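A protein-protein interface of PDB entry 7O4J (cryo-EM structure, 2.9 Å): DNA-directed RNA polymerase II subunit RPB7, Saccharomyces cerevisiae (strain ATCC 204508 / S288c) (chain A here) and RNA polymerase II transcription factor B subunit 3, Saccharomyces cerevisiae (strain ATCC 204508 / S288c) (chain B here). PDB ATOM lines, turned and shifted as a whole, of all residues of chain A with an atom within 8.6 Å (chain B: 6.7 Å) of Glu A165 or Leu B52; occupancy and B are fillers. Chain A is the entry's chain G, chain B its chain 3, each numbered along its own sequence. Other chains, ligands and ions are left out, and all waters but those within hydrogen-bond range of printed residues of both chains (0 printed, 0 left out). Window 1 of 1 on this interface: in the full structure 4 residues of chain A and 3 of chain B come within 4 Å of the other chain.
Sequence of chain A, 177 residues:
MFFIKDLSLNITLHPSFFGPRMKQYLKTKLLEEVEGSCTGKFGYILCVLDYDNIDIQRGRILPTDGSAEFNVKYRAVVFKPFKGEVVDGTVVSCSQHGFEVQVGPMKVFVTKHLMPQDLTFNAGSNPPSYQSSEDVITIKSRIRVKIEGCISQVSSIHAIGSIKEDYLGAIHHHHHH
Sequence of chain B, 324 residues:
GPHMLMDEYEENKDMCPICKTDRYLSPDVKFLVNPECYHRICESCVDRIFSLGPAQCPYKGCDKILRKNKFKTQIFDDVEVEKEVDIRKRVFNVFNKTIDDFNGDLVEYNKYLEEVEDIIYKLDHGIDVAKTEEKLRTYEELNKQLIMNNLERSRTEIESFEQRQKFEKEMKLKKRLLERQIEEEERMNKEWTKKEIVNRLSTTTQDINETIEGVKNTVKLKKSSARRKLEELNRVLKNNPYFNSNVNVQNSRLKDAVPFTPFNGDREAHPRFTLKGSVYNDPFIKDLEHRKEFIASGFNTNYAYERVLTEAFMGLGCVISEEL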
ATOM      1  N   GLY A  84     -30.645 -12.995  -7.259  1.00  0.00           N
ATOM      2  CA  GLY A  84     -29.276 -13.437  -7.112  1.00  0.00           C
ATOM      3  C   GLY A  84     -29.021 -14.853  -7.576  1.00  0.00           C
ATOM      4  O   GLY A  84     -27.870 -15.307  -7.520  1.00  0.00           O
ATOM      5  N   VAL A  86     -28.907 -17.815 -10.563  1.00  0.00           N
ATOM      6  CA  VAL A  86     -28.575 -17.906 -11.980  1.00  0.00           C
ATOM      7  C   VAL A  86     -29.349 -19.072 -12.575  1.00  0.00           C
ATOM      8  O   VAL A  86     -29.321 -20.185 -12.036  1.00  0.00           O
ATOM      9  CB  VAL A  86     -27.061 -18.079 -12.192  1.00  0.00           C
ATOM     10  CG1 VAL A  86     -26.771 -18.615 -13.587  1.00  0.00           C
ATOM     11  CG2 VAL A  86     -26.344 -16.759 -11.961  1.00  0.00           C
ATOM     12  N   LYS A 112     -32.595  -3.319 -21.006  1.00  0.00           N
ATOM     13  CA  LYS A 112     -31.398  -2.865 -21.706  1.00  0.00           C
ATOM     14  C   LYS A 112     -30.302  -2.477 -20.723  1.00  0.00           C
ATOM     15  O   LYS A 112     -29.129  -2.815 -20.921  1.00  0.00           O
ATOM     16  CB  LYS A 112     -31.718  -1.674 -22.614  1.00  0.00           C
ATOM     17  CG  LYS A 112     -33.104  -1.681 -23.244  1.00  0.00           C
ATOM     18  CD  LYS A 112     -33.244  -0.592 -24.301  1.00  0.00           C
ATOM     19  CE  LYS A 112     -32.826   0.777 -23.779  1.00  0.00           C
ATOM     20  NZ  LYS A 112     -33.449   1.097 -22.466  1.00  0.00           N
ATOM     21  N   HIS A 113     -30.665  -1.763 -19.657  1.00  0.00           N
ATOM     22  CA  HIS A 113     -29.683  -1.323 -18.675  1.00  0.00           C
ATOM     23  C   HIS A 113     -29.023  -2.480 -17.943  1.00  0.00           C
ATOM     24  O   HIS A 113     -27.958  -2.285 -17.348  1.00  0.00           O
ATOM     25  CB  HIS A 113     -30.346  -0.384 -17.668  1.00  0.00           C
ATOM     26  CG  HIS A 113     -30.897   0.863 -18.283  1.00  0.00           C
ATOM     27  ND1 HIS A 113     -31.989   0.859 -19.123  1.00  0.00           N
ATOM     28  CD2 HIS A 113     -30.503   2.156 -18.185  1.00  0.00           C
ATOM     29  CE1 HIS A 113     -32.246   2.094 -19.515  1.00  0.00           C
ATOM     30  NE2 HIS A 113     -31.360   2.900 -18.960  1.00  0.00           N
ATOM     31  N   LEU A 114     -29.619  -3.671 -17.971  1.00  0.00           N
ATOM     32  CA  LEU A 114     -29.029  -4.854 -17.363  1.00  0.00           C
ATOM     33  C   LEU A 114     -28.329  -5.734 -18.392  1.00  0.00           C
ATOM     34  O   LEU A 114     -28.020  -6.893 -18.097  1.00  0.00           O
ATOM     35  CB  LEU A 114     -30.100  -5.657 -16.619  1.00  0.00           C
ATOM     36  CG  LEU A 114     -30.509  -5.143 -15.232  1.00  0.00           C
ATOM     37  CD1 LEU A 114     -29.338  -5.141 -14.250  1.00  0.00           C
ATOM     38  CD2 LEU A 114     -31.126  -3.755 -15.330  1.00  0.00           C
ATOM     39  N   MET A 115     -28.084  -5.213 -19.585  1.00  0.00           N
ATOM     40  CA  MET A 115     -27.347  -5.870 -20.648  1.00  0.00           C
ATOM     41  C   MET A 115     -25.994  -5.198 -20.844  1.00  0.00           C
ATOM     42  O   MET A 115     -25.804  -4.035 -20.473  1.00  0.00           O
ATOM     43  CB  MET A 115     -28.147  -5.817 -21.955  1.00  0.00           C
ATOM     44  CG  MET A 115     -29.416  -6.647 -21.950  1.00  0.00           C
ATOM     45  SD  MET A 115     -30.445  -6.322 -23.395  1.00  0.00           S
ATOM     46  CE  MET A 115     -32.051  -6.833 -22.794  1.00  0.00           C
ATOM     47  N   PRO A 116     -25.027  -5.900 -21.426  1.00  0.00           N
ATOM     48  CA  PRO A 116     -23.732  -5.273 -21.702  1.00  0.00           C
ATOM     49  C   PRO A 116     -23.853  -4.176 -22.750  1.00  0.00           C
ATOM     50  O   PRO A 116     -24.749  -4.172 -23.597  1.00  0.00           O
ATOM     51  CB  PRO A 116     -22.869  -6.434 -22.204  1.00  0.00           C
ATOM     52  CG  PRO A 116     -23.821  -7.422 -22.748  1.00  0.00           C
ATOM     53  CD  PRO A 116     -25.127  -7.243 -22.021  1.00  0.00           C
ATOM     54  N   ARG A 144     -28.055 -17.563 -20.333  1.00  0.00           N
ATOM     55  CA  ARG A 144     -27.855 -17.746 -18.902  1.00  0.00           C
ATOM     56  C   ARG A 144     -28.076 -16.404 -18.216  1.00  0.00           C
ATOM     57  O   ARG A 144     -27.321 -15.454 -18.449  1.00  0.00           O
ATOM     58  CB  ARG A 144     -26.455 -18.285 -18.611  1.00  0.00           C
ATOM     59  CG  ARG A 144     -26.226 -18.661 -17.155  1.00  0.00           C
ATOM     60  CD  ARG A 144     -25.015 -19.564 -16.989  1.00  0.00           C
ATOM     61  NE  ARG A 144     -25.158 -20.818 -17.724  1.00  0.00           N
ATOM     62  CZ  ARG A 144     -24.482 -21.931 -17.450  1.00  0.00           C
ATOM     63  NH1 ARG A 144     -23.607 -21.958 -16.453  1.00  0.00           N
ATOM     64  NH2 ARG A 144     -24.683 -23.021 -18.175  1.00  0.00           N
ATOM     65  N   VAL A 145     -29.104 -16.328 -17.377  1.00  0.00           N
ATOM     66  CA  VAL A 145     -29.571 -15.071 -16.808  1.00  0.00           C
ATOM     67  C   VAL A 145     -29.504 -15.147 -15.290  1.00  0.00           C
ATOM     68  O   VAL A 145     -29.848 -16.172 -14.693  1.00  0.00           O
ATOM     69  CB  VAL A 145     -31.006 -14.747 -17.271  1.00  0.00           C
ATOM     70  CG1 VAL A 145     -31.506 -13.484 -16.600  1.00  0.00           C
ATOM     71  CG2 VAL A 145     -31.055 -14.608 -18.781  1.00  0.00           C
ATOM     72  N   LYS A 146     -29.059 -14.057 -14.674  1.00  0.00           N
ATOM     73  CA  LYS A 146     -29.029 -13.919 -13.223  1.00  0.00           C
ATOM     74  C   LYS A 146     -30.201 -13.044 -12.799  1.00  0.00           C
ATOM     75  O   LYS A 146     -30.278 -11.873 -13.186  1.00  0.00           O
ATOM     76  CB  LYS A 146     -27.705 -13.308 -12.765  1.00  0.00           C
ATOM     77  CG  LYS A 146     -27.541 -13.223 -11.258  1.00  0.00           C
ATOM     78  CD  LYS A 146     -26.355 -12.349 -10.886  1.00  0.00           C
ATOM     79  CE  LYS A 146     -26.159 -12.284  -9.382  1.00  0.00           C
ATOM     80  NZ  LYS A 146     -24.964 -11.478  -9.011  1.00  0.00           N
ATOM     81  N   GLU A 148     -32.170 -10.508 -11.059  1.00  0.00           N
ATOM     82  CA  GLU A 148     -31.783  -9.338 -10.283  1.00  0.00           C
ATOM     83  C   GLU A 148     -32.887  -8.841  -9.360  1.00  0.00           C
ATOM     84  O   GLU A 148     -32.591  -8.134  -8.391  1.00  0.00           O
ATOM     85  CB  GLU A 148     -31.366  -8.199 -11.221  1.00  0.00           C
ATOM     86  CG  GLU A 148     -29.908  -8.245 -11.662  1.00  0.00           C
ATOM     87  CD  GLU A 148     -28.936  -8.256 -10.497  1.00  0.00           C
ATOM     88  OE1 GLU A 148     -27.880  -8.913 -10.607  1.00  0.00           O
ATOM     89  OE2 GLU A 148     -29.229  -7.607  -9.470  1.00  0.00           O
ATOM     90  N   ILE A 160     -36.859  -9.847 -12.989  1.00  0.00           N
ATOM     91  CA  ILE A 160     -35.967  -9.183 -13.931  1.00  0.00           C
ATOM     92  C   ILE A 160     -34.574  -9.770 -13.761  1.00  0.00           C
ATOM     93  O   ILE A 160     -34.098  -9.949 -12.634  1.00  0.00           O
ATOM     94  CB  ILE A 160     -35.948  -7.655 -13.733  1.00  0.00           C
ATOM     95  CG1 ILE A 160     -35.518  -7.302 -12.305  1.00  0.00           C
ATOM     96  CG2 ILE A 160     -37.310  -7.070 -14.051  1.00  0.00           C
ATOM     97  CD1 ILE A 160     -35.522  -5.815 -12.014  1.00  0.00           C
ATOM     98  N   GLY A 161     -33.921 -10.072 -14.887  1.00  0.00           N
ATOM     99  CA  GLY A 161     -32.616 -10.690 -14.868  1.00  0.00           C
ATOM    100  C   GLY A 161     -31.590  -9.834 -15.588  1.00  0.00           C
ATOM    101  O   GLY A 161     -31.917  -8.818 -16.206  1.00  0.00           O
ATOM    102  N   SER A 162     -30.336 -10.269 -15.496  1.00  0.00           N
ATOM    103  CA  SER A 162     -29.213  -9.553 -16.077  1.00  0.00           C
ATOM    104  C   SER A 162     -28.251 -10.540 -16.723  1.00  0.00           C
ATOM    105  O   SER A 162     -28.173 -11.709 -16.336  1.00  0.00           O
ATOM    106  CB  SER A 162     -28.472  -8.726 -15.022  1.00  0.00           C
ATOM    107  OG  SER A 162     -28.002  -9.546 -13.969  1.00  0.00           O
ATOM    108  N   ILE A 163     -27.519 -10.050 -17.721  1.00  0.00           N
ATOM    109  CA  ILE A 163     -26.500 -10.843 -18.399  1.00  0.00           C
ATOM    110  C   ILE A 163     -25.200 -10.051 -18.470  1.00  0.00           C
ATOM    111  O   ILE A 163     -24.321 -10.352 -19.286  1.00  0.00           O
ATOM    112  CB  ILE A 163     -26.977 -11.268 -19.801  1.00  0.00           C
ATOM    113  CG1 ILE A 163     -27.247 -10.040 -20.672  1.00  0.00           C
ATOM    114  CG2 ILE A 163     -28.226 -12.125 -19.695  1.00  0.00           C
ATOM    115  CD1 ILE A 163     -27.652 -10.372 -22.092  1.00  0.00           C
ATOM    116  N   LYS A 164     -25.068  -9.032 -17.617  1.00  0.00           N
ATOM    117  CA  LYS A 164     -23.868  -8.201 -17.624  1.00  0.00           C
ATOM    118  C   LYS A 164     -22.676  -8.918 -17.001  1.00  0.00           C
ATOM    119  O   LYS A 164     -21.546  -8.778 -17.482  1.00  0.00           O
ATOM    120  CB  LYS A 164     -24.134  -6.890 -16.884  1.00  0.00           C
ATOM    121  CG  LYS A 164     -24.941  -5.882 -17.681  1.00  0.00           C
ATOM    122  CD  LYS A 164     -25.336  -4.683 -16.830  1.00  0.00           C
ATOM    123  CE  LYS A 164     -24.177  -3.717 -16.643  1.00  0.00           C
ATOM    124  NZ  LYS A 164     -23.802  -3.034 -17.912  1.00  0.00           N
ATOM    125  N   GLU A 165     -22.903  -9.682 -15.937  1.00  0.00           N
ATOM    126  CA  GLU A 165     -21.805 -10.315 -15.227  1.00  0.00           C
ATOM    127  C   GLU A 165     -21.136 -11.369 -16.109  1.00  0.00           C
ATOM    128  O   GLU A 165     -21.684 -11.822 -17.118  1.00  0.00           O
ATOM    129  CB  GLU A 165     -22.303 -10.944 -13.926  1.00  0.00           C
ATOM    130  CG  GLU A 165     -21.194 -11.379 -12.981  1.00  0.00           C
ATOM    131  CD  GLU A 165     -21.563 -11.200 -11.521  1.00  0.00           C
ATOM    132  OE1 GLU A 165     -22.769 -11.086 -11.217  1.00  0.00           O
ATOM    133  OE2 GLU A 165     -20.644 -11.172 -10.675  1.00  0.00           O
ATOM    134  N   ASP A 166     -19.926 -11.756 -15.715  1.00  0.00           N
ATOM    135  CA  ASP A 166     -19.164 -12.731 -16.476  1.00  0.00           C
ATOM    136  C   ASP A 166     -19.848 -14.095 -16.442  1.00  0.00           C
ATOM    137  O   ASP A 166     -20.593 -14.428 -15.517  1.00  0.00           O
ATOM    138  CB  ASP A 166     -17.743 -12.849 -15.926  1.00  0.00           C
ATOM    139  CG  ASP A 166     -16.840 -11.728 -16.398  1.00  0.00           C
ATOM    140  OD1 ASP A 166     -16.922 -11.354 -17.587  1.00  0.00           O
ATOM    141  OD2 ASP A 166     -16.045 -11.220 -15.579  1.00  0.00           O
ATOM    142  N   TYR A 167     -19.585 -14.886 -17.480  1.00  0.00           N
ATOM    143  CA  TYR A 167     -20.125 -16.236 -17.617  1.00  0.00           C
ATOM    144  C   TYR A 167     -21.642 -16.240 -17.769  1.00  0.00           C
ATOM    145  O   TYR A 167     -22.287 -17.268 -17.546  1.00  0.00           O
ATOM    146  CB  TYR A 167     -19.710 -17.116 -16.433  1.00  0.00           C
ATOM    147  CG  TYR A 167     -18.214 -17.274 -16.294  1.00  0.00           C
ATOM    148  CD1 TYR A 167     -17.485 -18.000 -17.225  1.00  0.00           C
ATOM    149  CD2 TYR A 167     -17.530 -16.694 -15.235  1.00  0.00           C
ATOM    150  CE1 TYR A 167     -16.117 -18.148 -17.104  1.00  0.00           C
ATOM    151  CE2 TYR A 167     -16.162 -16.835 -15.105  1.00  0.00           C
ATOM    152  CZ  TYR A 167     -15.460 -17.563 -16.042  1.00  0.00           C
ATOM    153  OH  TYR A 167     -14.098 -17.707 -15.918  1.00  0.00           O
ATOM    154  N   LEU A 168     -22.223 -15.107 -18.145  1.00  0.00           N
ATOM    155  CA  LEU A 168     -23.649 -14.982 -18.406  1.00  0.00           C
ATOM    156  C   LEU A 168     -23.871 -14.740 -19.896  1.00  0.00           C
ATOM    157  O   LEU A 168     -22.927 -14.577 -20.674  1.00  0.00           O
ATOM    158  CB  LEU A 168     -24.252 -13.849 -17.573  1.00  0.00           C
ATOM    159  CG  LEU A 168     -24.408 -14.086 -16.070  1.00  0.00           C
ATOM    160  CD1 LEU A 168     -25.068 -12.881 -15.418  1.00  0.00           C
ATOM    161  CD2 LEU A 168     -25.206 -15.346 -15.786  1.00  0.00           C
ATOM    162  N   GLY A 169     -25.141 -14.718 -20.291  1.00  0.00           N
ATOM    163  CA  GLY A 169     -25.497 -14.435 -21.667  1.00  0.00           C
ATOM    164  C   GLY A 169     -25.662 -15.678 -22.515  1.00  0.00           C
ATOM    165  O   GLY A 169     -26.117 -16.716 -22.027  1.00  0.00           O
ATOM    166  N   ALA A 170     -25.294 -15.582 -23.790  1.00  0.00           N
ATOM    167  CA  ALA A 170     -25.460 -16.700 -24.708  1.00  0.00           C
ATOM    168  C   ALA A 170     -24.655 -17.903 -24.233  1.00  0.00           C
ATOM    169  O   ALA A 170     -23.496 -17.770 -23.829  1.00  0.00           O
ATOM    170  CB  ALA A 170     -25.027 -16.296 -26.115  1.00  0.00           C
ATOM    171  N   ASP B  47     -19.483  -1.615  -4.224  1.00  0.00           N
ATOM    172  CA  ASP B  47     -20.791  -2.222  -4.444  1.00  0.00           C
ATOM    173  C   ASP B  47     -21.558  -1.513  -5.552  1.00  0.00           C
ATOM    174  O   ASP B  47     -22.152  -2.163  -6.419  1.00  0.00           O
ATOM    175  CB  ASP B  47     -21.598  -2.209  -3.146  1.00  0.00           C
ATOM    176  CG  ASP B  47     -21.317  -3.414  -2.272  1.00  0.00           C
ATOM    177  OD1 ASP B  47     -20.196  -3.960  -2.352  1.00  0.00           O
ATOM    178  OD2 ASP B  47     -22.217  -3.818  -1.506  1.00  0.00           O
ATOM    179  N   ARG B  48     -21.553  -0.179  -5.550  1.00  0.00           N
ATOM    180  CA  ARG B  48     -22.391   0.552  -6.496  1.00  0.00           C
ATOM    181  C   ARG B  48     -21.801   0.525  -7.902  1.00  0.00           C
ATOM    182  O   ARG B  48     -22.545   0.549  -8.890  1.00  0.00           O
ATOM    183  CB  ARG B  48     -22.586   1.993  -6.018  1.00  0.00           C
ATOM    184  CG  ARG B  48     -21.369   2.887  -6.181  1.00  0.00           C
ATOM    185  CD  ARG B  48     -21.654   4.303  -5.711  1.00  0.00           C
ATOM    186  NE  ARG B  48     -20.442   5.115  -5.656  1.00  0.00           N
ATOM    187  CZ  ARG B  48     -19.893   5.721  -6.704  1.00  0.00           C
ATOM    188  NH1 ARG B  48     -20.441   5.613  -7.907  1.00  0.00           N
ATOM    189  NH2 ARG B  48     -18.789   6.438  -6.548  1.00  0.00           N
ATOM    190  N   ILE B  49     -20.475   0.474  -8.016  1.00  0.00           N
ATOM    191  CA  ILE B  49     -19.852   0.555  -9.333  1.00  0.00           C
ATOM    192  C   ILE B  49     -19.723  -0.819  -9.981  1.00  0.00           C
ATOM    193  O   ILE B  49     -19.701  -0.924 -11.213  1.00  0.00           O
ATOM    194  CB  ILE B  49     -18.479   1.246  -9.233  1.00  0.00           C
ATOM    195  CG1 ILE B  49     -18.649   2.698  -8.780  1.00  0.00           C
ATOM    196  CG2 ILE B  49     -17.752   1.181 -10.573  1.00  0.00           C
ATOM    197  CD1 ILE B  49     -17.349   3.415  -8.484  1.00  0.00           C
ATOM    198  N   PHE B  50     -19.641  -1.888  -9.185  1.00  0.00           N
ATOM    199  CA  PHE B  50     -19.304  -3.205  -9.706  1.00  0.00           C
ATOM    200  C   PHE B  50     -20.332  -4.287  -9.401  1.00  0.00           C
ATOM    201  O   PHE B  50     -20.140  -5.427  -9.837  1.00  0.00           O
ATOM    202  CB  PHE B  50     -17.945  -3.658  -9.150  1.00  0.00           C
ATOM    203  CG  PHE B  50     -16.814  -2.727  -9.481  1.00  0.00           C
ATOM    204  CD1 PHE B  50     -16.186  -2.782 -10.715  1.00  0.00           C
ATOM    205  CD2 PHE B  50     -16.377  -1.794  -8.556  1.00  0.00           C
ATOM    206  CE1 PHE B  50     -15.145  -1.925 -11.016  1.00  0.00           C
ATOM    207  CE2 PHE B  50     -15.338  -0.935  -8.852  1.00  0.00           C
ATOM    208  CZ  PHE B  50     -14.721  -1.001 -10.083  1.00  0.00           C
ATOM    209  N   SER B  51     -21.408  -3.977  -8.674  1.00  0.00           N
ATOM    210  CA  SER B  51     -22.361  -5.016  -8.296  1.00  0.00           C
ATOM    211  C   SER B  51     -23.010  -5.644  -9.524  1.00  0.00           C
ATOM    212  O   SER B  51     -23.140  -6.870  -9.613  1.00  0.00           O
ATOM    213  CB  SER B  51     -23.428  -4.436  -7.365  1.00  0.00           C
ATOM    214  OG  SER B  51     -22.907  -4.232  -6.063  1.00  0.00           O
ATOM    215  N   LEU B  52     -23.424  -4.815 -10.485  1.00  0.00           N
ATOM    216  CA  LEU B  52     -24.112  -5.341 -11.658  1.00  0.00           C
ATOM    217  C   LEU B  52     -23.200  -6.229 -12.494  1.00  0.00           C
ATOM    218  O   LEU B  52     -23.649  -7.249 -13.029  1.00  0.00           O
ATOM    219  CB  LEU B  52     -24.653  -4.191 -12.509  1.00  0.00           C
ATOM    220  CG  LEU B  52     -25.959  -3.539 -12.045  1.00  0.00           C
ATOM    221  CD1 LEU B  52     -26.421  -2.503 -13.057  1.00  0.00           C
ATOM    222  CD2 LEU B  52     -27.053  -4.572 -11.809  1.00  0.00           C
ATOM    223  N   GLY B  53     -21.927  -5.867 -12.615  1.00  0.00           N
ATOM    224  CA  GLY B  53     -20.994  -6.639 -13.399  1.00  0.00           C
ATOM    225  C   GLY B  53     -19.678  -5.915 -13.601  1.00  0.00           C
ATOM    226  O   GLY B  53     -19.406  -4.887 -12.973  1.00  0.00           O
ATOM    227  N   PRO B  54     -18.830  -6.444 -14.481  1.00  0.00           N
ATOM    228  CA  PRO B  54     -17.530  -5.807 -14.716  1.00  0.00           C
ATOM    229  C   PRO B  54     -17.684  -4.406 -15.285  1.00  0.00           C
ATOM    230  O   PRO B  54     -18.586  -4.131 -16.079  1.00  0.00           O
ATOM    231  CB  PRO B  54     -16.848  -6.750 -15.715  1.00  0.00           C
ATOM    232  CG  PRO B  54     -17.968  -7.457 -16.394  1.00  0.00           C
ATOM    233  CD  PRO B  54     -19.043  -7.607 -15.359  1.00  0.00           C
ATOM    234  N   ARG B  67     -13.218  -6.905 -11.797  1.00  0.00           N
ATOM    235  CA  ARG B  67     -14.428  -7.492 -11.242  1.00  0.00           C
ATOM    236  C   ARG B  67     -14.455  -7.323  -9.727  1.00  0.00           C
ATOM    237  O   ARG B  67     -13.413  -7.293  -9.068  1.00  0.00           O
ATOM    238  CB  ARG B  67     -14.529  -8.977 -11.600  1.00  0.00           C
ATOM    239  CG  ARG B  67     -14.869  -9.246 -13.061  1.00  0.00           C
ATOM    240  CD  ARG B  67     -13.620  -9.345 -13.925  1.00  0.00           C
ATOM    241  NE  ARG B  67     -13.911  -9.916 -15.241  1.00  0.00           N
ATOM    242  CZ  ARG B  67     -14.087  -9.211 -16.357  1.00  0.00           C
ATOM    243  NH1 ARG B  67     -14.006  -7.886 -16.346  1.00  0.00           N
ATOM    244  NH2 ARG B  67     -14.346  -9.837 -17.497  1.00  0.00           N
ATOM    245  N   LYS B  68     -15.669  -7.214  -9.182  1.00  0.00           N
ATOM    246  CA  LYS B  68     -15.819  -7.010  -7.744  1.00  0.00           C
ATOM    247  C   LYS B  68     -15.273  -8.193  -6.953  1.00  0.00           C
ATOM    248  O   LYS B  68     -14.785  -8.026  -5.830  1.00  0.00           O
ATOM    249  CB  LYS B  68     -17.289  -6.778  -7.398  1.00  0.00           C
ATOM    250  CG  LYS B  68     -17.544  -6.557  -5.917  1.00  0.00           C
ATOM    251  CD  LYS B  68     -18.984  -6.148  -5.649  1.00  0.00           C
ATOM    252  CE  LYS B  68     -19.928  -7.338  -5.713  1.00  0.00           C
ATOM    253  NZ  LYS B  68     -19.658  -8.329  -4.636  1.00  0.00           N
ATOM    254  N   ASN B  69     -15.348  -9.397  -7.522  1.00  0.00           N
ATOM    255  CA  ASN B  69     -14.927 -10.593  -6.805  1.00  0.00           C
ATOM    256  C   ASN B  69     -13.429 -10.612  -6.521  1.00  0.00           C
ATOM    257  O   ASN B  69     -12.984 -11.418  -5.696  1.00  0.00           O
ATOM    258  CB  ASN B  69     -15.323 -11.834  -7.610  1.00  0.00           C
ATOM    259  CG  ASN B  69     -14.871 -13.125  -6.959  1.00  0.00           C
ATOM    260  OD1 ASN B  69     -14.871 -13.249  -5.734  1.00  0.00           O
ATOM    261  ND2 ASN B  69     -14.487 -14.099  -7.777  1.00  0.00           N
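The side-chain carboxylate (OD2) of Asp A166 lies within salt-bridge range of the guanidinium group (NE) of Arg B67 (2.5 Å).
Of the printed residues of chain B, Leu A114 touches Leu B52.
Gly A161 touches none of the printed residues of chain B.
Of the printed residues of chain B, Lys A164 touches Leu B52 (3.9 Å) and Pro B54 (3.5 Å).
Of chain B, only Leu B52 (3.9 Å) and Pro B54 (3.9 Å) come within 4 Å of Glu A165.
Of the printed residues of chain B, Asp A166 touches Arg B67 (2.5 Å).
No residue of chain A comes within 4 Å of Gly B53.
Printed residues of chain A within 4 Å of Pro B54: Lys A164 (3.5 Å) and Glu A165 (3.9 Å).
Of the printed residues of chain A, Arg B67 touches Asp A166.
Among the printed residues, merely in contact across the chains: Leu A114 with Leu B52 (3.4 Å), Lys A164 with Leu B52 (3.9 Å), Lys A164 with Pro B54 (3.5 Å), Glu A165 with Leu B52 (3.9 Å) and Glu A165 with Pro B54 (3.9 Å).
Hydrophobic or aromatic side chains of chain A that line the printed part of chain B: Leu A114.
Among the printed residues, 6 pairs touch across the chains.
Among the printed residues, Asp or Glu carboxylates within 4 Å of a Lys or Arg side-chain nitrogen of the other chain: Asp A166 with Arg B67 (2.5 Å).
N of Ile A163 is in hydrogen-bond range of O of Leu A114.
The backbone carbonyl oxygen of Met A115 sits at hydrogen-bond distance from the side-chain amino group of Lys A164, 3.4 Å away.
The side-chain carboxylate of Glu A165 is in salt-bridge range of the side-chain amino group of Lys A146 (3.1 Å).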
